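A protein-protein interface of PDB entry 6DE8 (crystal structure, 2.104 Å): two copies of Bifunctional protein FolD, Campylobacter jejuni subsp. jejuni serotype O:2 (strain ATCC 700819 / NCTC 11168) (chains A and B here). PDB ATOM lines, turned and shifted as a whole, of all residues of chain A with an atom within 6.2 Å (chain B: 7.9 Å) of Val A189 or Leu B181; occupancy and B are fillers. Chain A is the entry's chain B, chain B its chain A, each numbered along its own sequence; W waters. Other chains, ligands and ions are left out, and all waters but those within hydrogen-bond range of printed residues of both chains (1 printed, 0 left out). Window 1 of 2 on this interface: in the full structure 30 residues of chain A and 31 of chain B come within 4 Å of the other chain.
Val A187 touches its own counterpart, Val B187.
Val A187 touches Ser B188, and with the chains exchanged Ser A188 touches Val B187.
Val A187 touches Val B189, and with the chains exchanged Val A189 touches Val B187.
Ser B188 touches its own counterpart, Ser A188.
Positions printed for both chains: 163, 165, 174, 177, 187, 188 and 189.
Water W1 lies within hydrogen-bond range of the side-chain amide nitrogen (ND2) of Asn B132 (3.1 Å) and the backbone carbonyl oxygen (O) of Arg A174 (3.1 Å).
Val A189 touches just these residues of chain B: Leu B181 (3.7 Å), Thr B186 (3.4 Å) and Val B187 (2.9 Å).
Of the printed residues of chain B, Thr A194 touches Thr B186.
Leu B131 touches none of the printed residues of chain A.
Met B176 touches none of the printed residues of chain A.
Leu B181 touches just these residues of chain A: Arg A174, Val A189 and His A191.
Printed residues of chain A within 4 Å of Asn B182: Arg A174.
Of the printed residues of chain A, Thr B186 touches Val A189, Cys A190, His A191 and Thr A194.
Printed residues of chain A within 4 Å of Val B189: Val A187.
The nearest residue of chain A that does not touch Leu B181 is Ala A168 (4.3 Å).
The nearest printed residue of chain B that does not touch Arg A174 is Leu B131 (4.5 Å).
Among the printed residues, merely in contact across the chains: Arg A174 with Thr B178, Arg A174 with Leu B181, Val A187 with Val B187, Val A187 with Ser B188, Ser A188 with Val B187, Val A189 with Leu B181, Val A189 with Thr B186, Cys A190 with Thr B186, His A191 with Leu B181, His A191 with Gly B184 and His A191 with Thr B186.
Hydrophobic or aromatic side chains of chain B that line the printed part of chain A: Leu B181, Val B187 and Val B189.
Among the printed residues, no Asp or Glu carboxylate lies within 4 Å of a Lys or Arg side-chain nitrogen of the other chain.
The backbone carbonyl oxygen (O) of Leu B131 sits at hydrogen-bond distance from the side-chain amide nitrogen (ND2) of Asn B182 (3.1 Å).
The backbone carbonyl oxygen (O) of Lys B161 sits at hydrogen-bond distance from the backbone NH (N) of Thr B186, 2.8 Å away.
O of Arg B174 sits at hydrogen-bond distance from OG1 of Thr B178 (3.1 Å).
O of Thr B178 sits close to ND2 of Asn B182 (3.4 Å).
O of Ala A163 sits at hydrogen-bond distance from N of Ser A188 (2.9 Å).
O of Ile A165 lies within hydrogen-bond range of N of Cys A190 (2.7 Å).
O of Asn B132 lies within hydrogen-bond range of NH1 of Arg A174, 3.1 Å away.
OD1 of Asn B182 lies within hydrogen-bond range of NH2 of Arg A174, 2.8 Å away.
A ring nitrogen (NE2) of His A191 sits at hydrogen-bond distance from the backbone carbonyl oxygen (O) of Ala B185.
OG1 of Thr B186 sits at hydrogen-bond distance from OG1 of Thr A194 (2.8 Å).
The backbone carbonyl oxygen (O) of Val B187 lies within hydrogen-bond range of the backbone NH (N) of Val A189 (2.9 Å).
OG of Ser A188 lies within hydrogen-bond range of OG of Ser B188, at 2.7 Å.
The backbone NH (N) of Val B189 is in hydrogen-bond range of the backbone carbonyl oxygen (O) of Val A187, at 2.9 Å.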
ATOM      1  N   ALA A 163     -21.563  32.298 -25.318  1.00  0.00           N
ATOM      2  CA  ALA A 163     -20.812  32.692 -26.501  1.00  0.00           C
ATOM      3  C   ALA A 163     -19.747  31.653 -26.824  1.00  0.00           C
ATOM      4  O   ALA A 163     -19.079  31.130 -25.926  1.00  0.00           O
ATOM      5  CB  ALA A 163     -20.162  34.063 -26.301  1.00  0.00           C
ATOM      6  N   VAL A 164     -19.596  31.356 -28.112  1.00  0.00           N
ATOM      7  CA  VAL A 164     -18.580  30.434 -28.605  1.00  0.00           C
ATOM      8  C   VAL A 164     -17.692  31.186 -29.584  1.00  0.00           C
ATOM      9  O   VAL A 164     -18.189  31.792 -30.541  1.00  0.00           O
ATOM     10  CB  VAL A 164     -19.203  29.195 -29.274  1.00  0.00           C
ATOM     11  CG1 VAL A 164     -18.131  28.382 -29.982  1.00  0.00           C
ATOM     12  CG2 VAL A 164     -19.922  28.339 -28.243  1.00  0.00           C
ATOM     13  N   ILE A 165     -16.385  31.151 -29.342  1.00  0.00           N
ATOM     14  CA  ILE A 165     -15.398  31.801 -30.196  1.00  0.00           C
ATOM     15  C   ILE A 165     -14.629  30.712 -30.932  1.00  0.00           C
ATOM     16  O   ILE A 165     -13.978  29.869 -30.304  1.00  0.00           O
ATOM     17  CB  ILE A 165     -14.444  32.702 -29.393  1.00  0.00           C
ATOM     18  CG1 ILE A 165     -15.196  33.889 -28.780  1.00  0.00           C
ATOM     19  CG2 ILE A 165     -13.304  33.190 -30.274  1.00  0.00           C
ATOM     20  CD1 ILE A 165     -15.823  33.603 -27.428  1.00  0.00           C
ATOM     21  N   ILE A 166     -14.708  30.727 -32.258  1.00  0.00           N
ATOM     22  CA  ILE A 166     -14.025  29.755 -33.103  1.00  0.00           C
ATOM     23  C   ILE A 166     -12.770  30.426 -33.643  1.00  0.00           C
ATOM     24  O   ILE A 166     -12.847  31.345 -34.466  1.00  0.00           O
ATOM     25  CB  ILE A 166     -14.930  29.253 -34.234  1.00  0.00           C
ATOM     26  CG1 ILE A 166     -16.225  28.678 -33.657  1.00  0.00           C
ATOM     27  CG2 ILE A 166     -14.207  28.206 -35.064  1.00  0.00           C
ATOM     28  CD1 ILE A 166     -17.216  28.225 -34.708  1.00  0.00           C
ATOM     29  N   GLY A 167     -11.610  29.963 -33.185  1.00  0.00           N
ATOM     30  CA  GLY A 167     -10.354  30.623 -33.477  1.00  0.00           C
ATOM     31  C   GLY A 167      -9.782  31.280 -32.237  1.00  0.00           C
ATOM     32  O   GLY A 167     -10.498  31.986 -31.519  1.00  0.00           O
ATOM     33  N   ALA A 168      -8.500  31.054 -31.966  1.00  0.00           N
ATOM     34  CA  ALA A 168      -7.851  31.545 -30.756  1.00  0.00           C
ATOM     35  C   ALA A 168      -6.607  32.350 -31.097  1.00  0.00           C
ATOM     36  O   ALA A 168      -5.556  32.203 -30.465  1.00  0.00           O
ATOM     37  CB  ALA A 168      -7.505  30.393 -29.815  1.00  0.00           C
ATOM     38  N   GLY A 173      -9.403  36.097 -31.885  1.00  0.00           N
ATOM     39  CA  GLY A 173     -10.014  35.173 -30.945  1.00  0.00           C
ATOM     40  C   GLY A 173      -9.814  35.489 -29.475  1.00  0.00           C
ATOM     41  O   GLY A 173     -10.788  35.652 -28.734  1.00  0.00           O
ATOM     42  N   ARG A 174      -8.558  35.580 -29.042  1.00  0.00           N
ATOM     43  CA  ARG A 174      -8.281  35.794 -27.622  1.00  0.00           C
ATOM     44  C   ARG A 174      -8.807  37.126 -27.101  1.00  0.00           C
ATOM     45  O   ARG A 174      -9.466  37.129 -26.047  1.00  0.00           O
ATOM     46  CB  ARG A 174      -6.778  35.632 -27.369  1.00  0.00           C
ATOM     47  CG  ARG A 174      -6.316  34.187 -27.434  1.00  0.00           C
ATOM     48  CD  ARG A 174      -4.823  34.076 -27.679  1.00  0.00           C
ATOM     49  NE  ARG A 174      -4.398  32.681 -27.782  1.00  0.00           N
ATOM     50  CZ  ARG A 174      -3.808  32.005 -26.802  1.00  0.00           C
ATOM     51  NH1 ARG A 174      -3.563  32.597 -25.642  1.00  0.00           N
ATOM     52  NH2 ARG A 174      -3.457  30.738 -26.981  1.00  0.00           N
ATOM     53  N   ALA A 177     -12.760  36.870 -26.892  1.00  0.00           N
ATOM     54  CA  ALA A 177     -13.265  36.146 -25.732  1.00  0.00           C
ATOM     55  C   ALA A 177     -13.118  36.966 -24.458  1.00  0.00           C
ATOM     56  O   ALA A 177     -13.959  36.871 -23.556  1.00  0.00           O
ATOM     57  CB  ALA A 177     -12.540  34.809 -25.589  1.00  0.00           C
ATOM     58  N   VAL A 187     -17.978  32.330 -22.048  1.00  0.00           N
ATOM     59  CA  VAL A 187     -17.193  32.233 -23.272  1.00  0.00           C
ATOM     60  C   VAL A 187     -16.589  30.840 -23.386  1.00  0.00           C
ATOM     61  O   VAL A 187     -16.105  30.272 -22.402  1.00  0.00           O
ATOM     62  CB  VAL A 187     -16.095  33.316 -23.329  1.00  0.00           C
ATOM     63  CG1 VAL A 187     -16.726  34.693 -23.416  1.00  0.00           C
ATOM     64  CG2 VAL A 187     -15.181  33.228 -22.117  1.00  0.00           C
ATOM     65  N   SER A 188     -16.634  30.292 -24.598  1.00  0.00           N
ATOM     66  CA  SER A 188     -15.949  29.055 -24.952  1.00  0.00           C
ATOM     67  C   SER A 188     -15.051  29.346 -26.143  1.00  0.00           C
ATOM     68  O   SER A 188     -15.524  29.840 -27.171  1.00  0.00           O
ATOM     69  CB  SER A 188     -16.942  27.939 -25.289  1.00  0.00           C
ATOM     70  OG  SER A 188     -17.721  27.580 -24.161  1.00  0.00           O
ATOM     71  N   VAL A 189     -13.764  29.050 -26.003  1.00  0.00           N
ATOM     72  CA  VAL A 189     -12.782  29.294 -27.053  1.00  0.00           C
ATOM     73  C   VAL A 189     -12.458  27.957 -27.704  1.00  0.00           C
ATOM     74  O   VAL A 189     -11.851  27.080 -27.078  1.00  0.00           O
ATOM     75  CB  VAL A 189     -11.520  29.969 -26.503  1.00  0.00           C
ATOM     76  CG1 VAL A 189     -10.533  30.239 -27.628  1.00  0.00           C
ATOM     77  CG2 VAL A 189     -11.879  31.257 -25.782  1.00  0.00           C
ATOM     78  N   CYS A 190     -12.864  27.797 -28.960  1.00  0.00           N
ATOM     79  CA  CYS A 190     -12.585  26.603 -29.739  1.00  0.00           C
ATOM     80  C   CYS A 190     -11.532  26.907 -30.797  1.00  0.00           C
ATOM     81  O   CYS A 190     -11.313  28.062 -31.174  1.00  0.00           O
ATOM     82  CB  CYS A 190     -13.861  26.072 -30.402  1.00  0.00           C
ATOM     83  SG  CYS A 190     -15.202  25.713 -29.244  1.00  0.00           S
ATOM     84  N   HIS A 191     -10.882  25.851 -31.275  1.00  0.00           N
ATOM     85  CA  HIS A 191      -9.800  25.982 -32.242  1.00  0.00           C
ATOM     86  C   HIS A 191      -9.649  24.655 -32.979  1.00  0.00           C
ATOM     87  O   HIS A 191     -10.517  23.778 -32.897  1.00  0.00           O
ATOM     88  CB  HIS A 191      -8.505  26.417 -31.549  1.00  0.00           C
ATOM     89  CG  HIS A 191      -8.264  25.730 -30.241  1.00  0.00           C
ATOM     90  ND1 HIS A 191      -7.838  24.423 -30.155  1.00  0.00           N
ATOM     91  CD2 HIS A 191      -8.398  26.167 -28.966  1.00  0.00           C
ATOM     92  CE1 HIS A 191      -7.713  24.085 -28.883  1.00  0.00           C
ATOM     93  NE2 HIS A 191      -8.048  25.125 -28.141  1.00  0.00           N
ATOM     94  N   THR A 194      -9.996  21.395 -31.005  1.00  0.00           N
ATOM     95  CA  THR A 194     -11.262  21.045 -30.374  1.00  0.00           C
ATOM     96  C   THR A 194     -11.796  19.749 -30.969  1.00  0.00           C
ATOM     97  O   THR A 194     -11.826  19.581 -32.192  1.00  0.00           O
ATOM     98  CB  THR A 194     -12.275  22.174 -30.554  1.00  0.00           C
ATOM     99  OG1 THR A 194     -11.779  23.368 -29.936  1.00  0.00           O
ATOM    100  CG2 THR A 194     -13.611  21.801 -29.925  1.00  0.00           C
ATOM    101  N   LEU B 131       1.617  36.293 -21.134  1.00  0.00           N
ATOM    102  CA  LEU B 131       0.929  35.010 -21.043  1.00  0.00           C
ATOM    103  C   LEU B 131      -0.222  34.926 -22.037  1.00  0.00           C
ATOM    104  O   LEU B 131      -0.423  33.886 -22.676  1.00  0.00           O
ATOM    105  CB  LEU B 131       0.426  34.788 -19.617  1.00  0.00           C
ATOM    106  CG  LEU B 131      -0.536  33.617 -19.399  1.00  0.00           C
ATOM    107  CD1 LEU B 131       0.126  32.297 -19.760  1.00  0.00           C
ATOM    108  CD2 LEU B 131      -1.041  33.599 -17.964  1.00  0.00           C
ATOM    109  N   ASN B 132      -0.988  36.009 -22.183  1.00  0.00           N
ATOM    110  CA  ASN B 132      -2.111  35.993 -23.111  1.00  0.00           C
ATOM    111  C   ASN B 132      -1.641  35.934 -24.559  1.00  0.00           C
ATOM    112  O   ASN B 132      -2.374  35.454 -25.431  1.00  0.00           O
ATOM    113  CB  ASN B 132      -2.998  37.215 -22.881  1.00  0.00           C
ATOM    114  CG  ASN B 132      -4.410  37.014 -23.391  1.00  0.00           C
ATOM    115  OD1 ASN B 132      -4.753  37.435 -24.496  1.00  0.00           O
ATOM    116  ND2 ASN B 132      -5.240  36.362 -22.584  1.00  0.00           N
ATOM    117  N   GLY B 134       0.787  34.033 -25.408  1.00  0.00           N
ATOM    118  CA  GLY B 134       1.360  32.714 -25.562  1.00  0.00           C
ATOM    119  C   GLY B 134       2.842  32.633 -25.297  1.00  0.00           C
ATOM    120  O   GLY B 134       3.460  31.611 -25.620  1.00  0.00           O
ATOM    121  N   MET B 148      -0.974  23.636 -13.314  1.00  0.00           N
ATOM    122  CA  MET B 148      -0.348  23.109 -14.521  1.00  0.00           C
ATOM    123  C   MET B 148       0.809  22.172 -14.182  1.00  0.00           C
ATOM    124  O   MET B 148       0.939  21.098 -14.766  1.00  0.00           O
ATOM    125  CB  MET B 148       0.144  24.253 -15.410  1.00  0.00           C
ATOM    126  CG  MET B 148      -0.963  25.165 -15.915  1.00  0.00           C
ATOM    127  SD  MET B 148      -2.200  24.271 -17.133  1.00  0.00           S
ATOM    128  CE  MET B 148      -0.963  23.923 -18.599  1.00  0.00           C
ATOM    129  N   LEU B 158      -3.341  17.540 -21.884  1.00  0.00           N
ATOM    130  CA  LEU B 158      -4.379  18.556 -21.956  1.00  0.00           C
ATOM    131  C   LEU B 158      -4.759  18.924 -23.383  1.00  0.00           C
ATOM    132  O   LEU B 158      -5.756  19.628 -23.579  1.00  0.00           O
ATOM    133  CB  LEU B 158      -3.926  19.817 -21.209  1.00  0.00           C
ATOM    134  CG  LEU B 158      -3.435  19.602 -19.775  1.00  0.00           C
ATOM    135  CD1 LEU B 158      -2.753  20.850 -19.245  1.00  0.00           C
ATOM    136  CD2 LEU B 158      -4.584  19.194 -18.865  1.00  0.00           C
ATOM    137  N   LYS B 161      -8.438  18.534 -24.808  1.00  0.00           N
ATOM    138  CA  LYS B 161      -9.372  18.264 -23.727  1.00  0.00           C
ATOM    139  C   LYS B 161     -10.363  19.411 -23.569  1.00  0.00           C
ATOM    140  O   LYS B 161     -10.033  20.582 -23.783  1.00  0.00           O
ATOM    141  CB  LYS B 161      -8.622  18.038 -22.416  1.00  0.00           C
ATOM    142  CG  LYS B 161      -7.702  16.826 -22.421  1.00  0.00           C
ATOM    143  CD  LYS B 161      -8.462  15.536 -22.157  1.00  0.00           C
ATOM    144  CE  LYS B 161      -7.545  14.327 -22.267  1.00  0.00           C
ATOM    145  NZ  LYS B 161      -7.101  14.110 -23.672  1.00  0.00           N
ATOM    146  N   ASP B 162     -11.591  19.060 -23.197  1.00  0.00           N
ATOM    147  CA  ASP B 162     -12.639  20.038 -22.926  1.00  0.00           C
ATOM    148  C   ASP B 162     -12.523  20.475 -21.472  1.00  0.00           C
ATOM    149  O   ASP B 162     -12.886  19.724 -20.560  1.00  0.00           O
ATOM    150  CB  ASP B 162     -14.016  19.444 -23.212  1.00  0.00           C
ATOM    151  CG  ASP B 162     -14.182  19.025 -24.660  1.00  0.00           C
ATOM    152  OD1 ASP B 162     -13.722  19.765 -25.555  1.00  0.00           O
ATOM    153  OD2 ASP B 162     -14.770  17.948 -24.900  1.00  0.00           O
ATOM    154  N   ALA B 163     -12.017  21.684 -21.254  1.00  0.00           N
ATOM    155  CA  ALA B 163     -11.790  22.209 -19.917  1.00  0.00           C
ATOM    156  C   ALA B 163     -12.819  23.281 -19.591  1.00  0.00           C
ATOM    157  O   ALA B 163     -13.192  24.079 -20.456  1.00  0.00           O
ATOM    158  CB  ALA B 163     -10.378  22.783 -19.784  1.00  0.00           C
ATOM    159  N   ILE B 165     -13.529  26.260 -16.608  1.00  0.00           N
ATOM    160  CA  ILE B 165     -13.046  27.038 -15.472  1.00  0.00           C
ATOM    161  C   ILE B 165     -14.235  27.788 -14.890  1.00  0.00           C
ATOM    162  O   ILE B 165     -14.930  28.516 -15.610  1.00  0.00           O
ATOM    163  CB  ILE B 165     -11.925  28.010 -15.874  1.00  0.00           C
ATOM    164  CG1 ILE B 165     -10.684  27.253 -16.363  1.00  0.00           C
ATOM    165  CG2 ILE B 165     -11.564  28.928 -14.712  1.00  0.00           C
ATOM    166  CD1 ILE B 165     -10.650  27.018 -17.860  1.00  0.00           C
ATOM    167  N   ARG B 174      -8.781  33.708 -14.935  1.00  0.00           N
ATOM    168  CA  ARG B 174      -8.368  34.192 -16.251  1.00  0.00           C
ATOM    169  C   ARG B 174      -7.000  33.663 -16.664  1.00  0.00           C
ATOM    170  O   ARG B 174      -6.880  33.137 -17.785  1.00  0.00           O
ATOM    171  CB  ARG B 174      -8.438  35.723 -16.286  1.00  0.00           C
ATOM    172  CG  ARG B 174      -9.861  36.261 -16.239  1.00  0.00           C
ATOM    173  CD  ARG B 174      -9.901  37.754 -15.961  1.00  0.00           C
ATOM    174  NE  ARG B 174     -11.267  38.268 -15.992  1.00  0.00           N
ATOM    175  CZ  ARG B 174     -11.764  39.018 -16.969  1.00  0.00           C
ATOM    176  NH1 ARG B 174     -11.001  39.362 -17.999  1.00  0.00           N
ATOM    177  NH2 ARG B 174     -13.021  39.435 -16.912  1.00  0.00           N
ATOM    178  N   PRO B 175      -5.942  33.754 -15.845  1.00  0.00           N
ATOM    179  CA  PRO B 175      -4.665  33.154 -16.268  1.00  0.00           C
ATOM    180  C   PRO B 175      -4.722  31.642 -16.416  1.00  0.00           C
ATOM    181  O   PRO B 175      -3.946  31.080 -17.199  1.00  0.00           O
ATOM    182  CB  PRO B 175      -3.691  33.581 -15.160  1.00  0.00           C
ATOM    183  CG  PRO B 175      -4.554  33.864 -13.985  1.00  0.00           C
ATOM    184  CD  PRO B 175      -5.809  34.446 -14.549  1.00  0.00           C
ATOM    185  N   MET B 176      -5.612  30.969 -15.693  1.00  0.00           N
ATOM    186  CA  MET B 176      -5.767  29.521 -15.822  1.00  0.00           C
ATOM    187  C   MET B 176      -6.284  29.145 -17.206  1.00  0.00           C
ATOM    188  O   MET B 176      -5.742  28.254 -17.863  1.00  0.00           O
ATOM    189  CB  MET B 176      -6.719  28.977 -14.753  1.00  0.00           C
ATOM    190  CG  MET B 176      -6.935  27.473 -14.813  1.00  0.00           C
ATOM    191  SD  MET B 176      -5.531  26.463 -13.920  1.00  0.00           S
ATOM    192  CE  MET B 176      -5.922  26.995 -12.068  1.00  0.00           C
ATOM    193  N   ALA B 177      -7.342  29.833 -17.642  1.00  0.00           N
ATOM    194  CA  ALA B 177      -7.909  29.563 -18.959  1.00  0.00           C
ATOM    195  C   ALA B 177      -6.892  29.831 -20.060  1.00  0.00           C
ATOM    196  O   ALA B 177      -6.864  29.126 -21.075  1.00  0.00           O
ATOM    197  CB  ALA B 177      -9.168  30.402 -19.173  1.00  0.00           C
ATOM    198  N   THR B 178      -6.042  30.844 -19.874  1.00  0.00           N
ATOM    199  CA  THR B 178      -5.035  31.155 -20.884  1.00  0.00           C
ATOM    200  C   THR B 178      -3.980  30.058 -20.969  1.00  0.00           C
ATOM    201  O   THR B 178      -3.571  29.670 -22.069  1.00  0.00           O
ATOM    202  CB  THR B 178      -4.387  32.507 -20.581  1.00  0.00           C
ATOM    203  OG1 THR B 178      -5.401  33.519 -20.512  1.00  0.00           O
ATOM    204  CG2 THR B 178      -3.392  32.875 -21.667  1.00  0.00           C
ATOM    205  N   MET B 179      -3.536  29.539 -19.827  1.00  0.00           N
ATOM    206  CA  MET B 179      -2.538  28.471 -19.819  1.00  0.00           C
ATOM    207  C   MET B 179      -3.103  27.183 -20.407  1.00  0.00           C
ATOM    208  O   MET B 179      -2.415  26.474 -21.142  1.00  0.00           O
ATOM    209  CB  MET B 179      -2.026  28.213 -18.402  1.00  0.00           C
ATOM    210  CG  MET B 179      -1.280  29.385 -17.795  1.00  0.00           C
ATOM    211  SD  MET B 179      -0.530  28.958 -16.048  1.00  0.00           S
ATOM    212  CE  MET B 179      -0.182  30.773 -15.442  1.00  0.00           C
ATOM    213  N   LEU B 180      -4.357  26.880 -20.067  1.00  0.00           N
ATOM    214  CA  LEU B 180      -5.023  25.725 -20.660  1.00  0.00           C
ATOM    215  C   LEU B 180      -5.227  25.923 -22.157  1.00  0.00           C
ATOM    216  O   LEU B 180      -5.089  24.975 -22.940  1.00  0.00           O
ATOM    217  CB  LEU B 180      -6.360  25.471 -19.959  1.00  0.00           C
ATOM    218  CG  LEU B 180      -6.291  24.911 -18.533  1.00  0.00           C
ATOM    219  CD1 LEU B 180      -7.673  24.808 -17.893  1.00  0.00           C
ATOM    220  CD2 LEU B 180      -5.603  23.555 -18.537  1.00  0.00           C
ATOM    221  N   LEU B 181      -5.544  27.150 -22.572  1.00  0.00           N
ATOM    222  CA  LEU B 181      -5.668  27.445 -23.995  1.00  0.00           C
ATOM    223  C   LEU B 181      -4.315  27.354 -24.689  1.00  0.00           C
ATOM    224  O   LEU B 181      -4.209  26.792 -25.786  1.00  0.00           O
ATOM    225  CB  LEU B 181      -6.285  28.831 -24.182  1.00  0.00           C
ATOM    226  CG  LEU B 181      -6.711  29.238 -25.590  1.00  0.00           C
ATOM    227  CD1 LEU B 181      -7.728  28.250 -26.137  1.00  0.00           C
ATOM    228  CD2 LEU B 181      -7.282  30.647 -25.575  1.00  0.00           C
ATOM    229  N   ASN B 182      -3.269  27.902 -24.063  1.00  0.00           N
ATOM    230  CA  ASN B 182      -1.924  27.779 -24.616  1.00  0.00           C
ATOM    231  C   ASN B 182      -1.494  26.323 -24.726  1.00  0.00           C
ATOM    232  O   ASN B 182      -0.731  25.969 -25.633  1.00  0.00           O
ATOM    233  CB  ASN B 182      -0.927  28.558 -23.756  1.00  0.00           C
ATOM    234  CG  ASN B 182      -1.075  30.059 -23.905  1.00  0.00           C
ATOM    235  OD1 ASN B 182      -1.706  30.541 -24.845  1.00  0.00           O
ATOM    236  ND2 ASN B 182      -0.477  30.808 -22.985  1.00  0.00           N
ATOM    237  N   ALA B 183      -1.968  25.469 -23.820  1.00  0.00           N
ATOM    238  CA  ALA B 183      -1.632  24.050 -23.845  1.00  0.00           C
ATOM    239  C   ALA B 183      -2.438  23.264 -24.872  1.00  0.00           C
ATOM    240  O   ALA B 183      -2.193  22.064 -25.035  1.00  0.00           O
ATOM    241  CB  ALA B 183      -1.829  23.436 -22.456  1.00  0.00           C
ATOM    242  N   GLY B 184      -3.384  23.899 -25.559  1.00  0.00           N
ATOM    243  CA  GLY B 184      -4.134  23.252 -26.613  1.00  0.00           C
ATOM    244  C   GLY B 184      -5.490  22.708 -26.225  1.00  0.00           C
ATOM    245  O   GLY B 184      -6.085  21.967 -27.016  1.00  0.00           O
ATOM    246  N   ALA B 185      -6.000  23.048 -25.047  1.00  0.00           N
ATOM    247  CA  ALA B 185      -7.308  22.578 -24.621  1.00  0.00           C
ATOM    248  C   ALA B 185      -8.399  23.537 -25.077  1.00  0.00           C
ATOM    249  O   ALA B 185      -8.151  24.720 -25.321  1.00  0.00           O
ATOM    250  CB  ALA B 185      -7.355  22.424 -23.100  1.00  0.00           C
ATOM    251  N   THR B 186      -9.614  23.007 -25.202  1.00  0.00           N
ATOM    252  CA  THR B 186     -10.795  23.838 -25.402  1.00  0.00           C
ATOM    253  C   THR B 186     -11.280  24.314 -24.037  1.00  0.00           C
ATOM    254  O   THR B 186     -11.499  23.497 -23.137  1.00  0.00           O
ATOM    255  CB  THR B 186     -11.884  23.050 -26.127  1.00  0.00           C
ATOM    256  OG1 THR B 186     -11.350  22.499 -27.337  1.00  0.00           O
ATOM    257  CG2 THR B 186     -13.059  23.957 -26.469  1.00  0.00           C
ATOM    258  N   VAL B 187     -11.409  25.630 -23.864  1.00  0.00           N
ATOM    259  CA  VAL B 187     -11.677  26.216 -22.553  1.00  0.00           C
ATOM    260  C   VAL B 187     -13.023  26.927 -22.568  1.00  0.00           C
ATOM    261  O   VAL B 187     -13.388  27.584 -23.550  1.00  0.00           O
ATOM    262  CB  VAL B 187     -10.555  27.183 -22.113  1.00  0.00           C
ATOM    263  CG1 VAL B 187      -9.245  26.426 -21.941  1.00  0.00           C
ATOM    264  CG2 VAL B 187     -10.388  28.319 -23.112  1.00  0.00           C
ATOM    265  N   SER B 188     -13.761  26.786 -21.467  1.00  0.00           N
ATOM    266  CA  SER B 188     -14.996  27.519 -21.222  1.00  0.00           C
ATOM    267  C   SER B 188     -14.893  28.191 -19.862  1.00  0.00           C
ATOM    268  O   SER B 188     -14.607  27.529 -18.858  1.00  0.00           O
ATOM    269  CB  SER B 188     -16.220  26.595 -21.264  1.00  0.00           C
ATOM    270  OG  SER B 188     -16.364  25.976 -22.530  1.00  0.00           O
ATOM    271  N   VAL B 189     -15.116  29.500 -19.829  1.00  0.00           N
ATOM    272  CA  VAL B 189     -15.021  30.286 -18.605  1.00  0.00           C
ATOM    273  C   VAL B 189     -16.436  30.591 -18.142  1.00  0.00           C
ATOM    274  O   VAL B 189     -17.178  31.327 -18.802  1.00  0.00           O
ATOM    275  CB  VAL B 189     -14.207  31.570 -18.812  1.00  0.00           C
ATOM    276  CG1 VAL B 189     -14.107  32.346 -17.497  1.00  0.00           C
ATOM    277  CG2 VAL B 189     -12.826  31.228 -19.339  1.00  0.00           C
HETATM  278  O   HOH W   1      -7.691  35.457 -24.162  1.00  0.00           O
